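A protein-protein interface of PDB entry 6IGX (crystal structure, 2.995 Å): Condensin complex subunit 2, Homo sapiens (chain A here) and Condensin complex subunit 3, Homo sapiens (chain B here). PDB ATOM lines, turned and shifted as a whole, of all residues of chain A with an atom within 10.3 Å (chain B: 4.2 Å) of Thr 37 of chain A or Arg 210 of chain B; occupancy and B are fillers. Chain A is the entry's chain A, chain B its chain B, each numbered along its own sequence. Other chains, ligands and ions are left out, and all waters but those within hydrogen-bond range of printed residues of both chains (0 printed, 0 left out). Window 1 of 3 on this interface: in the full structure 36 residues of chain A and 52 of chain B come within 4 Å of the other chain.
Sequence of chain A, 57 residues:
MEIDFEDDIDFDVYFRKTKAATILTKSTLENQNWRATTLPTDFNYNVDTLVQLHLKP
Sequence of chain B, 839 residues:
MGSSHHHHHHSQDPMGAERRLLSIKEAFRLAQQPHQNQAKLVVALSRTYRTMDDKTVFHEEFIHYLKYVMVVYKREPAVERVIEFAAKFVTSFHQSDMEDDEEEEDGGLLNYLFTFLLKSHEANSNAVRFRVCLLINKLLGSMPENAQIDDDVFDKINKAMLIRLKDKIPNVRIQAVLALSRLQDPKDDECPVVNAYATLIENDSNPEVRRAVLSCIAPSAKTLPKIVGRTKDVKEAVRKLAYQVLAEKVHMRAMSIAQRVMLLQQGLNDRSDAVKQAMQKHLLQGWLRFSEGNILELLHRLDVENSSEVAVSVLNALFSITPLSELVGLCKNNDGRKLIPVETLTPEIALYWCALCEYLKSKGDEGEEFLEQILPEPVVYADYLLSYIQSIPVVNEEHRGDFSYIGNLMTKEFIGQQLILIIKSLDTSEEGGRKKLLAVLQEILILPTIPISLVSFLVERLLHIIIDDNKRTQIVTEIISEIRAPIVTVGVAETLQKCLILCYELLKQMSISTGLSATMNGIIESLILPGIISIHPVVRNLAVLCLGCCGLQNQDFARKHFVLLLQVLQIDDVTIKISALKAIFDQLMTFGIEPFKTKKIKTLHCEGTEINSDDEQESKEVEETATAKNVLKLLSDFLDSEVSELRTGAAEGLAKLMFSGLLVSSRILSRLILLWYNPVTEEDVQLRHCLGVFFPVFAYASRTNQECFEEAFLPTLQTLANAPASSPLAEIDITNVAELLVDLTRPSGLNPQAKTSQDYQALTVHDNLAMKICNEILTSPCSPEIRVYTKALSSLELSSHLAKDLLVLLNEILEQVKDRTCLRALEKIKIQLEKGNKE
The side-chain hydroxyl (OG1) of Thr 38 of chain A sits at hydrogen-bond distance from the backbone carbonyl oxygen (O) of Trp 34 of chain A (2.7 Å). The guanidinium group of Arg 230 of chain B is in salt-bridge range of the side-chain carboxylate of Asp 233 of chain B, at 2.6 Å. The backbone NH (N) of Asn 206 of chain B is in hydrogen-bond range of the side-chain carboxylate (OD1) of Asp 204 of chain B, 2.7 Å away. O of Asp 204 of chain B lies within hydrogen-bond range of NH1 of Arg 210 of chain B (2.9 Å). The guanidinium group (NH1) of Arg 210 of chain B lies within hydrogen-bond range of the backbone carbonyl oxygen (O) of Ser 205 of chain B (3.5 Å). The guanidinium group of Arg 210 of chain B lies within salt-bridge range of the side-chain carboxylate of Asp 233 of chain B.
Printed residues of chain B that touch a printed residue of chain A: Glu 202, Asp 204, Ser 205, Arg 210, Arg 230, Asp 233 and Val 234. Hydrophobic or aromatic side chains of chain B that line the printed part of chain A: Val 234. Hydrophobic or aromatic side chains of chain A that line the printed part of chain B: Trp 34 and Leu 39. Among the printed residues, 12 pairs touch across the chains.
Thr 37 of chain A touches just these residues of chain B: Glu 202 (3.1 Å), Asp 204 (3.8 Å), Arg 210 (3.4 Å), Arg 230 (3.2 Å), Asp 233 (3.4 Å) and Val 234 (2.4 Å). Of chain A, only Thr 37 comes within 4 Å of Arg 210 of chain B. Ser 205 of chain B touches just one residue of chain A: Gln 32 (3.7 Å). No residue of chain A comes within 4 Å of Pro 207 of chain B. No residue of chain A comes within 4 Å of Val 213 of chain B. No residue of chain A comes within 4 Å of Leu 214 of chain B. Of chain A, only Thr 37 comes within 4 Å of Asp 233 of chain B. Val 234 of chain B touches just these residues of chain A: Ala 36, Thr 37, Thr 38 and Leu 39. Printed residues of chain B within 4 Å of Gln 32 of chain A: Ser 205. Printed residues of chain B within 4 Å of Thr 38 of chain A: Arg 230 (3.0 Å) and Val 234 (3.7 Å). The nearest printed residue of chain B that does not touch Thr 37 of chain A is Ile 201 of chain B (5.4 Å). The nearest printed residue of chain B that does not touch Gln 32 of chain A is Asp 204 of chain B (4.9 Å).
The backbone carbonyl oxygen of Glu 202 of chain B is in hydrogen-bond range of the side-chain hydroxyl of Thr 37 of chain A (3.1 Å). The backbone NH (N) of Val 234 of chain B is in hydrogen-bond range of the backbone carbonyl oxygen (O) of Thr 37 of chain A, at 2.4 Å. OG1 of Thr 37 of chain A lies within hydrogen-bond range of NH1 of Arg 230 of chain B, at 3.2 Å.
Among the printed residues, merely in contact across the chains: Gln 32 of chain A with Ser 205 of chain B (3.7 Å), Trp 34 of chain A with Glu 202 of chain B (3.5 Å), Ala 36 of chain A with Val 234 of chain B (3.6 Å), Thr 37 of chain A with Asp 204 of chain B (3.8 Å), Thr 37 of chain A with Arg 210 of chain B (3.4 Å), Thr 37 of chain A with Asp 233 of chain B (3.4 Å), Thr 38 of chain A with Arg 230 of chain B (3.0 Å), Thr 38 of chain A with Val 234 of chain B (3.7 Å) and Leu 39 of chain A with Val 234 of chain B (3.7 Å).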
ATOM      1  N   GLN A  32       0.513   0.520   7.391  1.00  0.00           N
ATOM      2  CA  GLN A  32      -0.145   1.814   7.243  1.00  0.00           C
ATOM      3  C   GLN A  32       0.626   2.725   6.293  1.00  0.00           C
ATOM      4  O   GLN A  32       1.848   2.634   6.180  1.00  0.00           O
ATOM      5  CB  GLN A  32      -0.331   2.489   8.603  1.00  0.00           C
ATOM      6  CG  GLN A  32      -1.382   1.801   9.464  1.00  0.00           C
ATOM      7  CD  GLN A  32      -1.662   2.530  10.764  1.00  0.00           C
ATOM      8  OE1 GLN A  32      -0.794   3.209  11.313  1.00  0.00           O
ATOM      9  NE2 GLN A  32      -2.886   2.392  11.263  1.00  0.00           N
ATOM     10  N   ASN A  33      -0.104   3.610   5.624  1.00  0.00           N
ATOM     11  CA  ASN A  33       0.445   4.427   4.548  1.00  0.00           C
ATOM     12  C   ASN A  33       0.231   5.925   4.725  1.00  0.00           C
ATOM     13  O   ASN A  33      -0.591   6.365   5.529  1.00  0.00           O
ATOM     14  CB  ASN A  33      -0.143   3.993   3.206  1.00  0.00           C
ATOM     15  CG  ASN A  33       0.856   3.245   2.350  1.00  0.00           C
ATOM     16  OD1 ASN A  33       2.065   3.326   2.575  1.00  0.00           O
ATOM     17  ND2 ASN A  33       0.358   2.519   1.357  1.00  0.00           N
ATOM     18  N   TRP A  34       0.983   6.699   3.948  1.00  0.00           N
ATOM     19  CA  TRP A  34       0.928   8.153   3.997  1.00  0.00           C
ATOM     20  C   TRP A  34      -0.418   8.666   3.505  1.00  0.00           C
ATOM     21  O   TRP A  34      -0.750   9.837   3.694  1.00  0.00           O
ATOM     22  CB  TRP A  34       2.041   8.762   3.141  1.00  0.00           C
ATOM     23  CG  TRP A  34       2.113   8.172   1.761  1.00  0.00           C
ATOM     24  CD1 TRP A  34       2.546   6.922   1.421  1.00  0.00           C
ATOM     25  CD2 TRP A  34       1.714   8.804   0.538  1.00  0.00           C
ATOM     26  NE1 TRP A  34       2.454   6.743   0.062  1.00  0.00           N
ATOM     27  CE2 TRP A  34       1.946   7.880  -0.502  1.00  0.00           C
ATOM     28  CE3 TRP A  34       1.189  10.060   0.224  1.00  0.00           C
ATOM     29  CZ2 TRP A  34       1.670   8.179  -1.835  1.00  0.00           C
ATOM     30  CZ3 TRP A  34       0.916  10.352  -1.102  1.00  0.00           C
ATOM     31  CH2 TRP A  34       1.158   9.415  -2.114  1.00  0.00           C
ATOM     32  N   ARG A  35      -1.175   7.792   2.850  1.00  0.00           N
ATOM     33  CA  ARG A  35      -2.484   8.160   2.333  1.00  0.00           C
ATOM     34  C   ARG A  35      -3.327   8.700   3.482  1.00  0.00           C
ATOM     35  O   ARG A  35      -4.107   9.637   3.315  1.00  0.00           O
ATOM     36  CB  ARG A  35      -3.175   6.959   1.684  1.00  0.00           C
ATOM     37  CG  ARG A  35      -2.301   6.160   0.728  1.00  0.00           C
ATOM     38  CD  ARG A  35      -2.052   6.896  -0.579  1.00  0.00           C
ATOM     39  NE  ARG A  35      -0.877   6.376  -1.272  1.00  0.00           N
ATOM     40  CZ  ARG A  35      -0.878   5.277  -2.021  1.00  0.00           C
ATOM     41  NH1 ARG A  35      -1.995   4.580  -2.176  1.00  0.00           N
ATOM     42  NH2 ARG A  35       0.237   4.873  -2.615  1.00  0.00           N
ATOM     43  N   ALA A  36      -3.153   8.091   4.650  1.00  0.00           N
ATOM     44  CA  ALA A  36      -3.863   8.497   5.855  1.00  0.00           C
ATOM     45  C   ALA A  36      -3.413   9.862   6.368  1.00  0.00           C
ATOM     46  O   ALA A  36      -4.236  10.675   6.788  1.00  0.00           O
ATOM     47  CB  ALA A  36      -3.687   7.447   6.939  1.00  0.00           C
ATOM     48  N   THR A  37      -2.106  10.103   6.343  1.00  0.00           N
ATOM     49  CA  THR A  37      -1.528  11.342   6.868  1.00  0.00           C
ATOM     50  C   THR A  37      -1.589  12.534   5.909  1.00  0.00           C
ATOM     51  O   THR A  37      -1.708  13.679   6.346  1.00  0.00           O
ATOM     52  CB  THR A  37      -0.060  11.130   7.282  1.00  0.00           C
ATOM     53  OG1 THR A  37       0.753  10.961   6.113  1.00  0.00           O
ATOM     54  CG2 THR A  37       0.070   9.901   8.164  1.00  0.00           C
ATOM     55  N   THR A  38      -1.482  12.273   4.610  1.00  0.00           N
ATOM     56  CA  THR A  38      -1.418  13.348   3.619  1.00  0.00           C
ATOM     57  C   THR A  38      -2.789  13.722   3.057  1.00  0.00           C
ATOM     58  O   THR A  38      -3.700  12.895   3.002  1.00  0.00           O
ATOM     59  CB  THR A  38      -0.500  12.971   2.441  1.00  0.00           C
ATOM     60  OG1 THR A  38      -0.994  11.785   1.807  1.00  0.00           O
ATOM     61  CG2 THR A  38       0.916  12.725   2.925  1.00  0.00           C
ATOM     62  N   LEU A  39      -2.923  14.977   2.639  1.00  0.00           N
ATOM     63  CA  LEU A  39      -4.144  15.445   1.996  1.00  0.00           C
ATOM     64  C   LEU A  39      -4.138  15.140   0.501  1.00  0.00           C
ATOM     65  O   LEU A  39      -3.087  15.156  -0.138  1.00  0.00           O
ATOM     66  CB  LEU A  39      -4.318  16.949   2.215  1.00  0.00           C
ATOM     67  CG  LEU A  39      -4.772  17.408   3.599  1.00  0.00           C
ATOM     68  CD1 LEU A  39      -5.053  18.904   3.595  1.00  0.00           C
ATOM     69  CD2 LEU A  39      -6.004  16.628   4.029  1.00  0.00           C
ATOM     70  N   PRO A  40      -5.322  14.860  -0.061  1.00  0.00           N
ATOM     71  CA  PRO A  40      -5.479  14.643  -1.500  1.00  0.00           C
ATOM     72  C   PRO A  40      -5.627  15.966  -2.243  1.00  0.00           C
ATOM     73  O   PRO A  40      -6.458  16.788  -1.858  1.00  0.00           O
ATOM     74  CB  PRO A  40      -6.757  13.814  -1.584  1.00  0.00           C
ATOM     75  CG  PRO A  40      -7.570  14.313  -0.434  1.00  0.00           C
ATOM     76  CD  PRO A  40      -6.582  14.628   0.668  1.00  0.00           C
ATOM     77  N   LEU B 200       8.665   6.902   9.983  1.00  0.00           N
ATOM     78  CA  LEU B 200       7.741   7.447  10.973  1.00  0.00           C
ATOM     79  C   LEU B 200       7.090   8.757  10.541  1.00  0.00           C
ATOM     80  O   LEU B 200       5.897   8.961  10.760  1.00  0.00           O
ATOM     81  CB  LEU B 200       8.469   7.658  12.303  1.00  0.00           C
ATOM     82  CG  LEU B 200       8.466   6.480  13.276  1.00  0.00           C
ATOM     83  CD1 LEU B 200       9.409   6.737  14.439  1.00  0.00           C
ATOM     84  CD2 LEU B 200       7.058   6.217  13.777  1.00  0.00           C
ATOM     85  N   ILE B 201       7.877   9.643   9.937  1.00  0.00           N
ATOM     86  CA  ILE B 201       7.399  10.975   9.578  1.00  0.00           C
ATOM     87  C   ILE B 201       6.205  10.939   8.628  1.00  0.00           C
ATOM     88  O   ILE B 201       5.423  11.887   8.573  1.00  0.00           O
ATOM     89  CB  ILE B 201       8.520  11.817   8.934  1.00  0.00           C
ATOM     90  CG1 ILE B 201       8.104  13.287   8.848  1.00  0.00           C
ATOM     91  CG2 ILE B 201       8.883  11.272   7.563  1.00  0.00           C
ATOM     92  CD1 ILE B 201       9.262  14.238   8.653  1.00  0.00           C
ATOM     93  N   GLU B 202       6.063   9.846   7.884  1.00  0.00           N
ATOM     94  CA  GLU B 202       4.969   9.716   6.925  1.00  0.00           C
ATOM     95  C   GLU B 202       3.940   8.664   7.332  1.00  0.00           C
ATOM     96  O   GLU B 202       2.778   8.742   6.932  1.00  0.00           O
ATOM     97  CB  GLU B 202       5.512   9.378   5.535  1.00  0.00           C
ATOM     98  CG  GLU B 202       5.921  10.581   4.703  1.00  0.00           C
ATOM     99  CD  GLU B 202       6.415  10.193   3.321  1.00  0.00           C
ATOM    100  OE1 GLU B 202       6.552   8.979   3.054  1.00  0.00           O
ATOM    101  OE2 GLU B 202       6.667  11.103   2.503  1.00  0.00           O
ATOM    102  N   ASP B 204       3.290   7.192  10.665  1.00  0.00           N
ATOM    103  CA  ASP B 204       2.757   7.048  12.015  1.00  0.00           C
ATOM    104  C   ASP B 204       1.330   7.576  12.100  1.00  0.00           C
ATOM    105  O   ASP B 204       1.041   8.695  11.673  1.00  0.00           O
ATOM    106  CB  ASP B 204       3.641   7.761  13.037  1.00  0.00           C
ATOM    107  CG  ASP B 204       3.294   7.381  14.463  1.00  0.00           C
ATOM    108  OD1 ASP B 204       2.315   7.936  15.005  1.00  0.00           O
ATOM    109  OD2 ASP B 204       3.994   6.523  15.039  1.00  0.00           O
ATOM    110  N   SER B 205       0.444   6.751  12.644  1.00  0.00           N
ATOM    111  CA  SER B 205      -0.960   7.105  12.821  1.00  0.00           C
ATOM    112  C   SER B 205      -1.149   8.422  13.579  1.00  0.00           C
ATOM    113  O   SER B 205      -2.117   9.145  13.355  1.00  0.00           O
ATOM    114  CB  SER B 205      -1.690   5.974  13.547  1.00  0.00           C
ATOM    115  OG  SER B 205      -3.073   6.249  13.662  1.00  0.00           O
ATOM    116  N   ASN B 206      -0.215   8.726  14.473  1.00  0.00           N
ATOM    117  CA  ASN B 206      -0.370   9.845  15.396  1.00  0.00           C
ATOM    118  C   ASN B 206       0.351  11.102  14.920  1.00  0.00           C
ATOM    119  O   ASN B 206       1.556  11.076  14.672  1.00  0.00           O
ATOM    120  CB  ASN B 206       0.131   9.454  16.785  1.00  0.00           C
ATOM    121  CG  ASN B 206      -0.139  10.523  17.818  1.00  0.00           C
ATOM    122  OD1 ASN B 206       0.627  11.479  17.954  1.00  0.00           O
ATOM    123  ND2 ASN B 206      -1.231  10.368  18.556  1.00  0.00           N
ATOM    124  N   PRO B 207      -0.393  12.209  14.789  1.00  0.00           N
ATOM    125  CA  PRO B 207       0.112  13.489  14.271  1.00  0.00           C
ATOM    126  C   PRO B 207       1.307  14.037  15.050  1.00  0.00           C
ATOM    127  O   PRO B 207       2.232  14.574  14.443  1.00  0.00           O
ATOM    128  CB  PRO B 207      -1.095  14.428  14.415  1.00  0.00           C
ATOM    129  CG  PRO B 207      -2.281  13.527  14.473  1.00  0.00           C
ATOM    130  CD  PRO B 207      -1.811  12.291  15.176  1.00  0.00           C
ATOM    131  N   GLU B 208       1.287  13.902  16.372  1.00  0.00           N
ATOM    132  CA  GLU B 208       2.372  14.417  17.204  1.00  0.00           C
ATOM    133  C   GLU B 208       3.662  13.627  17.014  1.00  0.00           C
ATOM    134  O   GLU B 208       4.752  14.202  17.038  1.00  0.00           O
ATOM    135  CB  GLU B 208       1.966  14.425  18.679  1.00  0.00           C
ATOM    136  CG  GLU B 208       1.060  15.592  19.059  1.00  0.00           C
ATOM    137  CD  GLU B 208      -0.408  15.324  18.773  1.00  0.00           C
ATOM    138  OE1 GLU B 208      -0.751  14.167  18.444  1.00  0.00           O
ATOM    139  OE2 GLU B 208      -1.216  16.273  18.871  1.00  0.00           O
ATOM    140  N   VAL B 209       3.539  12.314  16.845  1.00  0.00           N
ATOM    141  CA  VAL B 209       4.695  11.477  16.542  1.00  0.00           C
ATOM    142  C   VAL B 209       5.378  11.985  15.282  1.00  0.00           C
ATOM    143  O   VAL B 209       6.599  12.133  15.245  1.00  0.00           O
ATOM    144  CB  VAL B 209       4.308  10.002  16.353  1.00  0.00           C
ATOM    145  CG1 VAL B 209       5.485   9.221  15.775  1.00  0.00           C
ATOM    146  CG2 VAL B 209       3.860   9.399  17.676  1.00  0.00           C
ATOM    147  N   ARG B 210       4.581  12.247  14.252  1.00  0.00           N
ATOM    148  CA  ARG B 210       5.093  12.804  13.006  1.00  0.00           C
ATOM    149  C   ARG B 210       5.666  14.199  13.241  1.00  0.00           C
ATOM    150  O   ARG B 210       6.814  14.477  12.889  1.00  0.00           O
ATOM    151  CB  ARG B 210       3.990  12.863  11.947  1.00  0.00           C
ATOM    152  CG  ARG B 210       3.349  11.521  11.631  1.00  0.00           C
ATOM    153  CD  ARG B 210       2.411  11.624  10.439  1.00  0.00           C
ATOM    154  NE  ARG B 210       1.405  12.670  10.609  1.00  0.00           N
ATOM    155  CZ  ARG B 210       0.152  12.448  10.990  1.00  0.00           C
ATOM    156  NH1 ARG B 210      -0.257  11.212  11.245  1.00  0.00           N
ATOM    157  NH2 ARG B 210      -0.694  13.461  11.117  1.00  0.00           N
ATOM    158  N   ARG B 211       4.856  15.073  13.832  1.00  0.00           N
ATOM    159  CA  ARG B 211       5.291  16.422  14.178  1.00  0.00           C
ATOM    160  C   ARG B 211       6.577  16.407  15.003  1.00  0.00           C
ATOM    161  O   ARG B 211       7.382  17.335  14.939  1.00  0.00           O
ATOM    162  CB  ARG B 211       4.193  17.164  14.942  1.00  0.00           C
ATOM    163  CG  ARG B 211       4.506  18.635  15.163  1.00  0.00           C
ATOM    164  CD  ARG B 211       3.632  19.253  16.241  1.00  0.00           C
ATOM    165  NE  ARG B 211       4.055  20.616  16.547  1.00  0.00           N
ATOM    166  CZ  ARG B 211       5.144  20.922  17.246  1.00  0.00           C
ATOM    167  NH1 ARG B 211       5.929  19.957  17.709  1.00  0.00           N
ATOM    168  NH2 ARG B 211       5.455  22.192  17.478  1.00  0.00           N
ATOM    169  N   ALA B 212       6.762  15.346  15.780  1.00  0.00           N
ATOM    170  CA  ALA B 212       7.979  15.176  16.561  1.00  0.00           C
ATOM    171  C   ALA B 212       9.159  14.878  15.645  1.00  0.00           C
ATOM    172  O   ALA B 212      10.200  15.532  15.724  1.00  0.00           O
ATOM    173  CB  ALA B 212       7.806  14.067  17.583  1.00  0.00           C
ATOM    174  N   VAL B 213       8.991  13.880  14.782  1.00  0.00           N
ATOM    175  CA  VAL B 213      10.039  13.480  13.854  1.00  0.00           C
ATOM    176  C   VAL B 213      10.389  14.605  12.885  1.00  0.00           C
ATOM    177  O   VAL B 213      11.510  14.674  12.380  1.00  0.00           O
ATOM    178  CB  VAL B 213       9.623  12.237  13.045  1.00  0.00           C
ATOM    179  CG1 VAL B 213      10.741  11.820  12.094  1.00  0.00           C
ATOM    180  CG2 VAL B 213       9.255  11.094  13.978  1.00  0.00           C
ATOM    181  N   LEU B 214       9.427  15.488  12.637  1.00  0.00           N
ATOM    182  CA  LEU B 214       9.618  16.586  11.698  1.00  0.00           C
ATOM    183  C   LEU B 214      10.537  17.669  12.251  1.00  0.00           C
ATOM    184  O   LEU B 214      11.170  18.402  11.491  1.00  0.00           O
ATOM    185  CB  LEU B 214       8.266  17.198  11.322  1.00  0.00           C
ATOM    186  CG  LEU B 214       8.291  18.404  10.379  1.00  0.00           C
ATOM    187  CD1 LEU B 214       9.087  18.087   9.121  1.00  0.00           C
ATOM    188  CD2 LEU B 214       6.881  18.851  10.029  1.00  0.00           C
ATOM    189  N   ARG B 230       5.708  17.005   4.150  1.00  0.00           N
ATOM    190  CA  ARG B 230       4.884  17.239   5.328  1.00  0.00           C
ATOM    191  C   ARG B 230       4.137  18.560   5.218  1.00  0.00           C
ATOM    192  O   ARG B 230       3.381  18.929   6.114  1.00  0.00           O
ATOM    193  CB  ARG B 230       5.731  17.209   6.601  1.00  0.00           C
ATOM    194  CG  ARG B 230       5.981  15.806   7.114  1.00  0.00           C
ATOM    195  CD  ARG B 230       4.679  15.022   7.151  1.00  0.00           C
ATOM    196  NE  ARG B 230       4.552  14.131   6.002  1.00  0.00           N
ATOM    197  CZ  ARG B 230       3.416  13.552   5.624  1.00  0.00           C
ATOM    198  NH1 ARG B 230       2.297  13.775   6.298  1.00  0.00           N
ATOM    199  NH2 ARG B 230       3.398  12.756   4.565  1.00  0.00           N
ATOM    200  N   ASP B 233       0.668  17.407   4.922  1.00  0.00           N
ATOM    201  CA  ASP B 233       0.162  16.610   6.033  1.00  0.00           C
ATOM    202  C   ASP B 233      -1.269  17.009   6.376  1.00  0.00           C
ATOM    203  O   ASP B 233      -1.645  18.172   6.240  1.00  0.00           O
ATOM    204  CB  ASP B 233       1.065  16.763   7.258  1.00  0.00           C
ATOM    205  CG  ASP B 233       0.699  15.803   8.375  1.00  0.00           C
ATOM    206  OD1 ASP B 233      -0.247  16.098   9.134  1.00  0.00           O
ATOM    207  OD2 ASP B 233       1.362  14.751   8.490  1.00  0.00           O
ATOM    208  N   VAL B 234      -2.064  16.039   6.812  1.00  0.00           N
ATOM    209  CA  VAL B 234      -3.458  16.292   7.158  1.00  0.00           C
ATOM    210  C   VAL B 234      -3.588  17.304   8.293  1.00  0.00           C
ATOM    211  O   VAL B 234      -4.512  18.119   8.306  1.00  0.00           O
ATOM    212  CB  VAL B 234      -4.184  14.990   7.563  1.00  0.00           C
ATOM    213  CG1 VAL B 234      -5.416  15.303   8.395  1.00  0.00           C
ATOM    214  CG2 VAL B 234      -4.561  14.184   6.329  1.00  0.00           C
